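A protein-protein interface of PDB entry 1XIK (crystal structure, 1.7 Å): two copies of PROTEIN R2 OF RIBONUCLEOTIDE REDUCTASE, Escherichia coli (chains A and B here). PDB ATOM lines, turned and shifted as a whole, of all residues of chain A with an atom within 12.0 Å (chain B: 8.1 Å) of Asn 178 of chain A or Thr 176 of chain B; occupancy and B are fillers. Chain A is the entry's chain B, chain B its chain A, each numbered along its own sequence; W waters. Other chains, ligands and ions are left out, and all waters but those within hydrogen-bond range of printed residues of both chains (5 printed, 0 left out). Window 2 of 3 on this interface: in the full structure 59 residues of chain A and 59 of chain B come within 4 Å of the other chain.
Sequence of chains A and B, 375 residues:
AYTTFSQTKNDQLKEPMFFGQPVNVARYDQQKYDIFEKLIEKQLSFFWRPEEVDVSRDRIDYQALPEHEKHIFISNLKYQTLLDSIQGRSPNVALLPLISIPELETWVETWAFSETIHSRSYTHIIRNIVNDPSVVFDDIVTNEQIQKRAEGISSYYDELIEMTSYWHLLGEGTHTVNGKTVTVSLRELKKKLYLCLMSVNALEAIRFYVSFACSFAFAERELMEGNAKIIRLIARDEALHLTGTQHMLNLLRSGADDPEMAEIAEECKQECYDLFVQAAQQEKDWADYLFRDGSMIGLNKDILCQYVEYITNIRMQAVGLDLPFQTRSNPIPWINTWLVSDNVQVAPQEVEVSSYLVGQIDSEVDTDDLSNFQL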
ATOM      1  N   TYR A 166     -15.320 -19.174 -32.448  1.00  0.00           N
ATOM      2  CA  TYR A 166     -15.953 -17.887 -32.301  1.00  0.00           C
ATOM      3  C   TYR A 166     -15.809 -17.059 -33.566  1.00  0.00           C
ATOM      4  O   TYR A 166     -16.711 -16.311 -33.973  1.00  0.00           O
ATOM      5  CB  TYR A 166     -15.350 -17.119 -31.122  1.00  0.00           C
ATOM      6  CG  TYR A 166     -16.035 -17.388 -29.785  1.00  0.00           C
ATOM      7  CD1 TYR A 166     -17.293 -16.844 -29.491  1.00  0.00           C
ATOM      8  CD2 TYR A 166     -15.412 -18.164 -28.812  1.00  0.00           C
ATOM      9  CE1 TYR A 166     -17.893 -17.080 -28.287  1.00  0.00           C
ATOM     10  CE2 TYR A 166     -16.017 -18.407 -27.602  1.00  0.00           C
ATOM     11  CZ  TYR A 166     -17.259 -17.865 -27.346  1.00  0.00           C
ATOM     12  OH  TYR A 166     -17.866 -18.097 -26.130  1.00  0.00           O
ATOM     13  N   LEU A 169     -18.256 -18.443 -36.177  1.00  0.00           N
ATOM     14  CA  LEU A 169     -19.651 -18.239 -35.835  1.00  0.00           C
ATOM     15  C   LEU A 169     -20.046 -16.775 -35.797  1.00  0.00           C
ATOM     16  O   LEU A 169     -21.075 -16.412 -36.364  1.00  0.00           O
ATOM     17  CB  LEU A 169     -19.926 -18.798 -34.456  1.00  0.00           C
ATOM     18  CG  LEU A 169     -20.407 -20.233 -34.358  1.00  0.00           C
ATOM     19  CD1 LEU A 169     -20.062 -21.098 -35.554  1.00  0.00           C
ATOM     20  CD2 LEU A 169     -19.902 -20.739 -33.055  1.00  0.00           C
ATOM     21  N   LEU A 170     -19.282 -15.937 -35.098  1.00  0.00           N
ATOM     22  CA  LEU A 170     -19.632 -14.517 -34.936  1.00  0.00           C
ATOM     23  C   LEU A 170     -18.898 -13.525 -35.815  1.00  0.00           C
ATOM     24  O   LEU A 170     -19.347 -12.388 -35.986  1.00  0.00           O
ATOM     25  CB  LEU A 170     -19.406 -14.073 -33.497  1.00  0.00           C
ATOM     26  CG  LEU A 170     -20.335 -14.375 -32.326  1.00  0.00           C
ATOM     27  CD1 LEU A 170     -21.506 -15.190 -32.704  1.00  0.00           C
ATOM     28  CD2 LEU A 170     -19.732 -14.756 -30.958  1.00  0.00           C
ATOM     29  N   THR A 174     -17.020  -6.973 -31.449  1.00  0.00           N
ATOM     30  CA  THR A 174     -17.261  -7.067 -30.004  1.00  0.00           C
ATOM     31  C   THR A 174     -18.698  -7.549 -29.969  1.00  0.00           C
ATOM     32  O   THR A 174     -19.531  -6.956 -30.638  1.00  0.00           O
ATOM     33  CB  THR A 174     -17.212  -5.710 -29.333  1.00  0.00           C
ATOM     34  OG1 THR A 174     -15.900  -5.184 -29.514  1.00  0.00           O
ATOM     35  CG2 THR A 174     -17.466  -5.898 -27.844  1.00  0.00           C
ATOM     36  N   HIS A 175     -18.992  -8.631 -29.260  1.00  0.00           N
ATOM     37  CA  HIS A 175     -20.333  -9.193 -29.278  1.00  0.00           C
ATOM     38  C   HIS A 175     -20.684  -9.530 -27.875  1.00  0.00           C
ATOM     39  O   HIS A 175     -19.879  -9.356 -26.965  1.00  0.00           O
ATOM     40  CB  HIS A 175     -20.267 -10.551 -30.000  1.00  0.00           C
ATOM     41  CG  HIS A 175     -19.678 -10.497 -31.379  1.00  0.00           C
ATOM     42  ND1 HIS A 175     -18.370 -10.849 -31.650  1.00  0.00           N
ATOM     43  CD2 HIS A 175     -20.222 -10.163 -32.570  1.00  0.00           C
ATOM     44  CE1 HIS A 175     -18.134 -10.740 -32.944  1.00  0.00           C
ATOM     45  NE2 HIS A 175     -19.247 -10.334 -33.525  1.00  0.00           N
ATOM     46  N   THR A 176     -21.886 -10.066 -27.708  1.00  0.00           N
ATOM     47  CA  THR A 176     -22.319 -10.436 -26.371  1.00  0.00           C
ATOM     48  C   THR A 176     -22.787 -11.860 -26.343  1.00  0.00           C
ATOM     49  O   THR A 176     -23.391 -12.343 -27.287  1.00  0.00           O
ATOM     50  CB  THR A 176     -23.391  -9.447 -25.785  1.00  0.00           C
ATOM     51  OG1 THR A 176     -24.559  -9.391 -26.626  1.00  0.00           O
ATOM     52  CG2 THR A 176     -22.822  -8.021 -25.703  1.00  0.00           C
ATOM     53  N   VAL A 177     -22.519 -12.528 -25.239  1.00  0.00           N
ATOM     54  CA  VAL A 177     -22.946 -13.893 -25.133  1.00  0.00           C
ATOM     55  C   VAL A 177     -23.279 -14.065 -23.686  1.00  0.00           C
ATOM     56  O   VAL A 177     -22.435 -13.857 -22.840  1.00  0.00           O
ATOM     57  CB  VAL A 177     -21.805 -14.844 -25.527  1.00  0.00           C
ATOM     58  CG1 VAL A 177     -22.156 -16.274 -25.175  1.00  0.00           C
ATOM     59  CG2 VAL A 177     -21.471 -14.640 -26.982  1.00  0.00           C
ATOM     60  N   ASN A 178     -24.530 -14.397 -23.407  1.00  0.00           N
ATOM     61  CA  ASN A 178     -24.995 -14.604 -22.049  1.00  0.00           C
ATOM     62  C   ASN A 178     -24.667 -13.573 -20.972  1.00  0.00           C
ATOM     63  O   ASN A 178     -24.291 -13.934 -19.847  1.00  0.00           O
ATOM     64  CB  ASN A 178     -24.734 -16.035 -21.587  1.00  0.00           C
ATOM     65  CG  ASN A 178     -25.328 -17.061 -22.531  1.00  0.00           C
ATOM     66  OD1 ASN A 178     -26.434 -16.903 -23.037  1.00  0.00           O
ATOM     67  ND2 ASN A 178     -24.607 -18.124 -22.766  1.00  0.00           N
ATOM     68  N   GLY A 179     -24.802 -12.299 -21.315  1.00  0.00           N
ATOM     69  CA  GLY A 179     -24.534 -11.251 -20.337  1.00  0.00           C
ATOM     70  C   GLY A 179     -23.080 -10.778 -20.272  1.00  0.00           C
ATOM     71  O   GLY A 179     -22.782  -9.799 -19.592  1.00  0.00           O
ATOM     72  N   LYS A 180     -22.203 -11.444 -21.020  1.00  0.00           N
ATOM     73  CA  LYS A 180     -20.766 -11.104 -21.062  1.00  0.00           C
ATOM     74  C   LYS A 180     -20.293 -10.685 -22.462  1.00  0.00           C
ATOM     75  O   LYS A 180     -20.779 -11.222 -23.461  1.00  0.00           O
ATOM     76  CB  LYS A 180     -19.888 -12.257 -20.503  1.00  0.00           C
ATOM     77  CG  LYS A 180     -20.103 -13.689 -21.032  1.00  0.00           C
ATOM     78  CD  LYS A 180     -20.751 -14.572 -19.936  1.00  0.00           C
ATOM     79  CE  LYS A 180     -21.592 -15.771 -20.461  1.00  0.00           C
ATOM     80  NZ  LYS A 180     -22.690 -16.226 -19.524  1.00  0.00           N
ATOM     81  N   THR A 181     -19.334  -9.755 -22.538  1.00  0.00           N
ATOM     82  CA  THR A 181     -18.773  -9.312 -23.824  1.00  0.00           C
ATOM     83  C   THR A 181     -17.732 -10.292 -24.367  1.00  0.00           C
ATOM     84  O   THR A 181     -16.932 -10.833 -23.607  1.00  0.00           O
ATOM     85  CB  THR A 181     -18.174  -7.941 -23.683  1.00  0.00           C
ATOM     86  OG1 THR A 181     -19.182  -7.093 -23.116  1.00  0.00           O
ATOM     87  CG2 THR A 181     -17.727  -7.413 -25.037  1.00  0.00           C
ATOM     88  N   VAL A 182     -17.753 -10.566 -25.665  1.00  0.00           N
ATOM     89  CA  VAL A 182     -16.806 -11.504 -26.248  1.00  0.00           C
ATOM     90  C   VAL A 182     -16.277 -10.770 -27.457  1.00  0.00           C
ATOM     91  O   VAL A 182     -17.018 -10.505 -28.393  1.00  0.00           O
ATOM     92  CB  VAL A 182     -17.505 -12.760 -26.713  1.00  0.00           C
ATOM     93  CG1 VAL A 182     -16.671 -13.514 -27.735  1.00  0.00           C
ATOM     94  CG2 VAL A 182     -17.884 -13.618 -25.500  1.00  0.00           C
ATOM     95  N   THR A 183     -14.997 -10.391 -27.388  1.00  0.00           N
ATOM     96  CA  THR A 183     -14.303  -9.668 -28.463  1.00  0.00           C
ATOM     97  C   THR A 183     -13.638 -10.692 -29.363  1.00  0.00           C
ATOM     98  O   THR A 183     -13.069 -11.682 -28.902  1.00  0.00           O
ATOM     99  CB  THR A 183     -13.221  -8.750 -27.890  1.00  0.00           C
ATOM    100  OG1 THR A 183     -13.766  -7.970 -26.813  1.00  0.00           O
ATOM    101  CG2 THR A 183     -12.680  -7.832 -29.000  1.00  0.00           C
ATOM    102  N   LEU B 169     -18.830 -24.287 -27.716  1.00  0.00           N
ATOM    103  CA  LEU B 169     -18.682 -22.982 -27.089  1.00  0.00           C
ATOM    104  C   LEU B 169     -19.650 -22.691 -25.914  1.00  0.00           C
ATOM    105  O   LEU B 169     -19.256 -22.246 -24.818  1.00  0.00           O
ATOM    106  CB  LEU B 169     -18.882 -21.878 -28.130  1.00  0.00           C
ATOM    107  CG  LEU B 169     -17.795 -21.889 -29.178  1.00  0.00           C
ATOM    108  CD1 LEU B 169     -18.036 -20.685 -30.036  1.00  0.00           C
ATOM    109  CD2 LEU B 169     -16.466 -21.752 -28.449  1.00  0.00           C
ATOM    110  N   LEU B 170     -20.940 -22.906 -26.166  1.00  0.00           N
ATOM    111  CA  LEU B 170     -21.960 -22.587 -25.185  1.00  0.00           C
ATOM    112  C   LEU B 170     -22.529 -23.713 -24.358  1.00  0.00           C
ATOM    113  O   LEU B 170     -23.077 -23.449 -23.294  1.00  0.00           O
ATOM    114  CB  LEU B 170     -23.100 -21.834 -25.879  1.00  0.00           C
ATOM    115  CG  LEU B 170     -22.688 -20.858 -26.966  1.00  0.00           C
ATOM    116  CD1 LEU B 170     -23.933 -20.340 -27.654  1.00  0.00           C
ATOM    117  CD2 LEU B 170     -21.925 -19.698 -26.325  1.00  0.00           C
ATOM    118  N   GLY B 171     -22.457 -24.950 -24.825  1.00  0.00           N
ATOM    119  CA  GLY B 171     -23.049 -26.043 -24.067  1.00  0.00           C
ATOM    120  C   GLY B 171     -24.573 -26.033 -24.344  1.00  0.00           C
ATOM    121  O   GLY B 171     -25.140 -25.125 -24.916  1.00  0.00           O
ATOM    122  N   GLU B 172     -25.239 -27.084 -23.948  1.00  0.00           N
ATOM    123  CA  GLU B 172     -26.663 -27.207 -24.175  1.00  0.00           C
ATOM    124  C   GLU B 172     -27.475 -26.145 -23.488  1.00  0.00           C
ATOM    125  O   GLU B 172     -27.158 -25.763 -22.372  1.00  0.00           O
ATOM    126  CB  GLU B 172     -27.089 -28.462 -23.456  1.00  0.00           C
ATOM    127  CG  GLU B 172     -26.870 -29.672 -24.307  1.00  0.00           C
ATOM    128  CD  GLU B 172     -27.863 -30.743 -23.934  1.00  0.00           C
ATOM    129  OE1 GLU B 172     -29.045 -30.584 -24.360  1.00  0.00           O
ATOM    130  OE2 GLU B 172     -27.452 -31.684 -23.210  1.00  0.00           O
ATOM    131  N   GLY B 173     -28.566 -25.715 -24.113  1.00  0.00           N
ATOM    132  CA  GLY B 173     -29.422 -24.692 -23.511  1.00  0.00           C
ATOM    133  C   GLY B 173     -29.884 -23.588 -24.466  1.00  0.00           C
ATOM    134  O   GLY B 173     -29.772 -23.712 -25.690  1.00  0.00           O
ATOM    135  N   THR B 174     -30.424 -22.509 -23.911  1.00  0.00           N
ATOM    136  CA  THR B 174     -30.859 -21.435 -24.786  1.00  0.00           C
ATOM    137  C   THR B 174     -29.982 -20.343 -24.312  1.00  0.00           C
ATOM    138  O   THR B 174     -29.758 -20.176 -23.127  1.00  0.00           O
ATOM    139  CB  THR B 174     -32.366 -21.013 -24.683  1.00  0.00           C
ATOM    140  OG1 THR B 174     -32.732 -20.785 -23.317  1.00  0.00           O
ATOM    141  CG2 THR B 174     -33.247 -22.090 -25.259  1.00  0.00           C
ATOM    142  N   HIS B 175     -29.492 -19.594 -25.262  1.00  0.00           N
ATOM    143  CA  HIS B 175     -28.538 -18.585 -24.924  1.00  0.00           C
ATOM    144  C   HIS B 175     -28.912 -17.352 -25.687  1.00  0.00           C
ATOM    145  O   HIS B 175     -29.767 -17.381 -26.563  1.00  0.00           O
ATOM    146  CB  HIS B 175     -27.190 -19.169 -25.449  1.00  0.00           C
ATOM    147  CG  HIS B 175     -26.765 -20.440 -24.750  1.00  0.00           C
ATOM    148  ND1 HIS B 175     -26.799 -21.683 -25.354  1.00  0.00           N
ATOM    149  CD2 HIS B 175     -26.257 -20.658 -23.514  1.00  0.00           C
ATOM    150  CE1 HIS B 175     -26.339 -22.607 -24.527  1.00  0.00           C
ATOM    151  NE2 HIS B 175     -26.029 -22.009 -23.395  1.00  0.00           N
ATOM    152  N   THR B 176     -28.255 -16.264 -25.318  1.00  0.00           N
ATOM    153  CA  THR B 176     -28.484 -14.974 -25.926  1.00  0.00           C
ATOM    154  C   THR B 176     -27.132 -14.577 -26.527  1.00  0.00           C
ATOM    155  O   THR B 176     -26.131 -14.344 -25.814  1.00  0.00           O
ATOM    156  CB  THR B 176     -28.938 -13.949 -24.858  1.00  0.00           C
ATOM    157  OG1 THR B 176     -30.133 -14.397 -24.194  1.00  0.00           O
ATOM    158  CG2 THR B 176     -29.144 -12.582 -25.454  1.00  0.00           C
ATOM    159  N   VAL B 177     -27.115 -14.491 -27.853  1.00  0.00           N
ATOM    160  CA  VAL B 177     -25.920 -14.130 -28.603  1.00  0.00           C
ATOM    161  C   VAL B 177     -26.239 -12.860 -29.380  1.00  0.00           C
ATOM    162  O   VAL B 177     -27.098 -12.851 -30.240  1.00  0.00           O
ATOM    163  CB  VAL B 177     -25.514 -15.334 -29.511  1.00  0.00           C
ATOM    164  CG1 VAL B 177     -24.317 -15.011 -30.407  1.00  0.00           C
ATOM    165  CG2 VAL B 177     -25.335 -16.618 -28.706  1.00  0.00           C
ATOM    166  N   ASN B 178     -25.557 -11.773 -29.070  1.00  0.00           N
ATOM    167  CA  ASN B 178     -25.817 -10.487 -29.719  1.00  0.00           C
ATOM    168  C   ASN B 178     -27.296 -10.114 -29.695  1.00  0.00           C
ATOM    169  O   ASN B 178     -27.848  -9.628 -30.673  1.00  0.00           O
ATOM    170  CB  ASN B 178     -25.299 -10.471 -31.148  1.00  0.00           C
ATOM    171  CG  ASN B 178     -23.794 -10.403 -31.209  1.00  0.00           C
ATOM    172  OD1 ASN B 178     -23.146  -9.850 -30.307  1.00  0.00           O
ATOM    173  ND2 ASN B 178     -23.225 -11.011 -32.255  1.00  0.00           N
ATOM    174  N   GLY B 179     -27.955 -10.328 -28.575  1.00  0.00           N
ATOM    175  CA  GLY B 179     -29.365  -9.986 -28.574  1.00  0.00           C
ATOM    176  C   GLY B 179     -30.287 -11.000 -29.282  1.00  0.00           C
ATOM    177  O   GLY B 179     -31.483 -10.729 -29.398  1.00  0.00           O
ATOM    178  N   LYS B 180     -29.787 -12.157 -29.738  1.00  0.00           N
ATOM    179  CA  LYS B 180     -30.632 -13.195 -30.367  1.00  0.00           C
ATOM    180  C   LYS B 180     -30.633 -14.473 -29.528  1.00  0.00           C
ATOM    181  O   LYS B 180     -29.641 -14.812 -28.884  1.00  0.00           O
ATOM    182  CB  LYS B 180     -30.179 -13.585 -31.771  1.00  0.00           C
ATOM    183  CG  LYS B 180     -30.032 -12.416 -32.723  1.00  0.00           C
ATOM    184  CD  LYS B 180     -31.196 -12.310 -33.712  1.00  0.00           C
ATOM    185  CE  LYS B 180     -31.749 -10.869 -33.851  1.00  0.00           C
ATOM    186  NZ  LYS B 180     -30.779  -9.763 -34.196  1.00  0.00           N
ATOM    187  N   THR B 181     -31.753 -15.196 -29.544  1.00  0.00           N
ATOM    188  CA  THR B 181     -31.811 -16.427 -28.764  1.00  0.00           C
ATOM    189  C   THR B 181     -31.239 -17.510 -29.646  1.00  0.00           C
ATOM    190  O   THR B 181     -31.481 -17.564 -30.855  1.00  0.00           O
ATOM    191  CB  THR B 181     -33.228 -16.817 -28.314  1.00  0.00           C
ATOM    192  OG1 THR B 181     -33.758 -15.789 -27.475  1.00  0.00           O
ATOM    193  CG2 THR B 181     -33.175 -18.078 -27.494  1.00  0.00           C
ATOM    194  N   VAL B 182     -30.437 -18.356 -29.025  1.00  0.00           N
ATOM    195  CA  VAL B 182     -29.810 -19.439 -29.753  1.00  0.00           C
ATOM    196  C   VAL B 182     -30.021 -20.616 -28.836  1.00  0.00           C
ATOM    197  O   VAL B 182     -29.753 -20.584 -27.624  1.00  0.00           O
ATOM    198  CB  VAL B 182     -28.287 -19.199 -29.965  1.00  0.00           C
ATOM    199  CG1 VAL B 182     -27.646 -20.376 -30.645  1.00  0.00           C
ATOM    200  CG2 VAL B 182     -28.069 -18.027 -30.878  1.00  0.00           C
ATOM    201  N   THR B 183     -30.542 -21.667 -29.443  1.00  0.00           N
ATOM    202  CA  THR B 183     -30.787 -22.844 -28.651  1.00  0.00           C
ATOM    203  C   THR B 183     -29.782 -23.931 -28.990  1.00  0.00           C
ATOM    204  O   THR B 183     -29.516 -24.198 -30.153  1.00  0.00           O
ATOM    205  CB  THR B 183     -32.166 -23.369 -28.958  1.00  0.00           C
ATOM    206  OG1 THR B 183     -33.080 -22.394 -28.453  1.00  0.00           O
ATOM    207  CG2 THR B 183     -32.393 -24.677 -28.232  1.00  0.00           C
HETATM  208  O   HOH W   1     -24.690  -7.722 -28.407  1.00  0.00           O
HETATM  209  O   HOH W   2     -22.518 -11.583 -35.435  1.00  0.00           O
HETATM  210  O   HOH W   3     -29.583 -16.070 -21.830  1.00  0.00           O
HETATM  211  O   HOH W   4     -16.670 -20.939 -24.515  1.00  0.00           O
HETATM  212  O   HOH W   5     -26.330 -11.294 -26.104  1.00  0.00           O
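Water W1 lies within hydrogen-bond range of OG1 of Thr 176 of chain A (2.4 Å) and OD1 of Asn 178 of chain B (3.2 Å). Water W5 lies within hydrogen-bond range of OG1 of Thr 176 of chain A (2.7 Å), O of Thr 176 of chain B (3.1 Å), N of Asn 178 of chain B (3.1 Å) and N of Gly 179 of chain B (3.1 Å). Water W4 bridges the backbone carbonyl oxygen (O) of Leu 169 of chain B (2.9 Å) and the side-chain hydroxyl (OH) of Tyr 166 of chain A (3.5 Å). Water W3 lies within hydrogen-bond range of OG1 of Thr 176 of chain B (2.9 Å) and OD1 of Asn 178 of chain A (3.5 Å). Water W2 bridges ND2 of Asn 178 of chain B (3.3 Å) and O of Leu 170 of chain A (3.3 Å).
Hydrophobic or aromatic side chains of chain B within 4 Å of the printed part of chain A: Leu 169, Leu 170, His 175 and Val 177. Of the 13 printed residues of chain A, 7 touch a printed residue of chain B. Hydrophobic or aromatic side chains of chain A within 4 Å of the printed part of chain B: Tyr 166, Leu 169, Leu 170, His 175 and Val 177.
Leu 169 of chain A touches its own counterpart, Leu 169 of chain B. Leu 170 of chain A touches Val 177 of chain B, and with the chains exchanged Val 177 of chain A touches Leu 170 of chain B. Thr 176 of chain A touches Val 177 of chain B, and with the chains exchanged Val 177 of chain A touches Thr 176 of chain B. Thr 176 of chain A touches Asn 178 of chain B, and with the chains exchanged Asn 178 of chain A touches Thr 176 of chain B. 12 positions are printed for both chains. Of the 11 pairs that touch across the chains among the printed residues, 10 have their exchanged pair printed and touching as well.
The backbone carbonyl oxygen (O) of Thr 176 of chain A sits at hydrogen-bond distance from the backbone NH (N) of Asn 178 of chain B (2.9 Å). The backbone NH (N) of Asn 178 of chain A is in hydrogen-bond range of the backbone carbonyl oxygen (O) of Thr 176 of chain B, 2.9 Å away.
Among the printed residues, pairs that only touch across the chains: Tyr 166 of chain A with Leu 169 of chain B (3.5 Å), Leu 169 of chain A with Leu 169 of chain B (3.5 Å), Leu 170 of chain A with Val 177 of chain B (3.6 Å), His 175 of chain A with Asn 178 of chain B (3.0 Å), Thr 176 of chain A with Thr 176 of chain B (3.7 Å), Thr 176 of chain A with Val 177 of chain B (3.4 Å), Val 177 of chain A with Leu 170 of chain B (3.6 Å), Val 177 of chain A with Thr 176 of chain B (3.3 Å) and Asn 178 of chain A with His 175 of chain B (3.1 Å).
Of chain B, only His 175 and Thr 176 come within 4 Å of Asn 178 of chain A. Thr 176 of chain B touches just these residues of chain A: Thr 176 (3.7 Å), Val 177 (3.3 Å) and Asn 178 (2.9 Å). Leu 170 of chain B touches just one residue of chain A: Val 177 (3.6 Å). Of chain A, only Asn 178 (3.1 Å) comes within 4 Å of His 175 of chain B. Val 177 of chain B touches just these residues of chain A: Leu 170 (3.6 Å) and Thr 176 (3.4 Å). Asn 178 of chain B touches two residues of chain A. No residue of chain A comes within 4 Å of Gly 179 of chain B. No residue of chain A comes within 4 Å of Thr 181 of chain B. No residue of chain A comes within 4 Å of Val 182 of chain B. Printed residues of chain B within 4 Å of Leu 170 of chain A: Val 177. Of the printed residues of chain A, Leu 169 of chain B touches Tyr 166 (3.5 Å) and Leu 169 (3.5 Å). Thr 183 of chain A touches none of the printed residues of chain B. Thr 181 of chain A touches none of the printed residues of chain B. The nearest residue of chain B that does not touch Asn 178 of chain A is Thr 174 of chain B (4.7 Å). The nearest residue of chain A that does not touch Thr 176 of chain B is Gly 179 of chain A (5.1 Å).
The backbone carbonyl oxygen (O) of Leu 170 of chain B sits at hydrogen-bond distance from a ring nitrogen (NE2) of His 175 of chain B. N of Val 182 of chain A sits at hydrogen-bond distance from O of His 175 of chain A (2.8 Å). O of Asn 178 of chain A lies within hydrogen-bond range of NZ of Lys 180 of chain A. The backbone carbonyl oxygen (O) of Val 182 of chain B lies within hydrogen-bond range of the backbone NH (N) of His 175 of chain B, at 2.6 Å. The backbone carbonyl oxygen (O) of Leu 170 of chain A lies within hydrogen-bond range of a ring nitrogen (NE2) of His 175 of chain A, 3.2 Å away.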
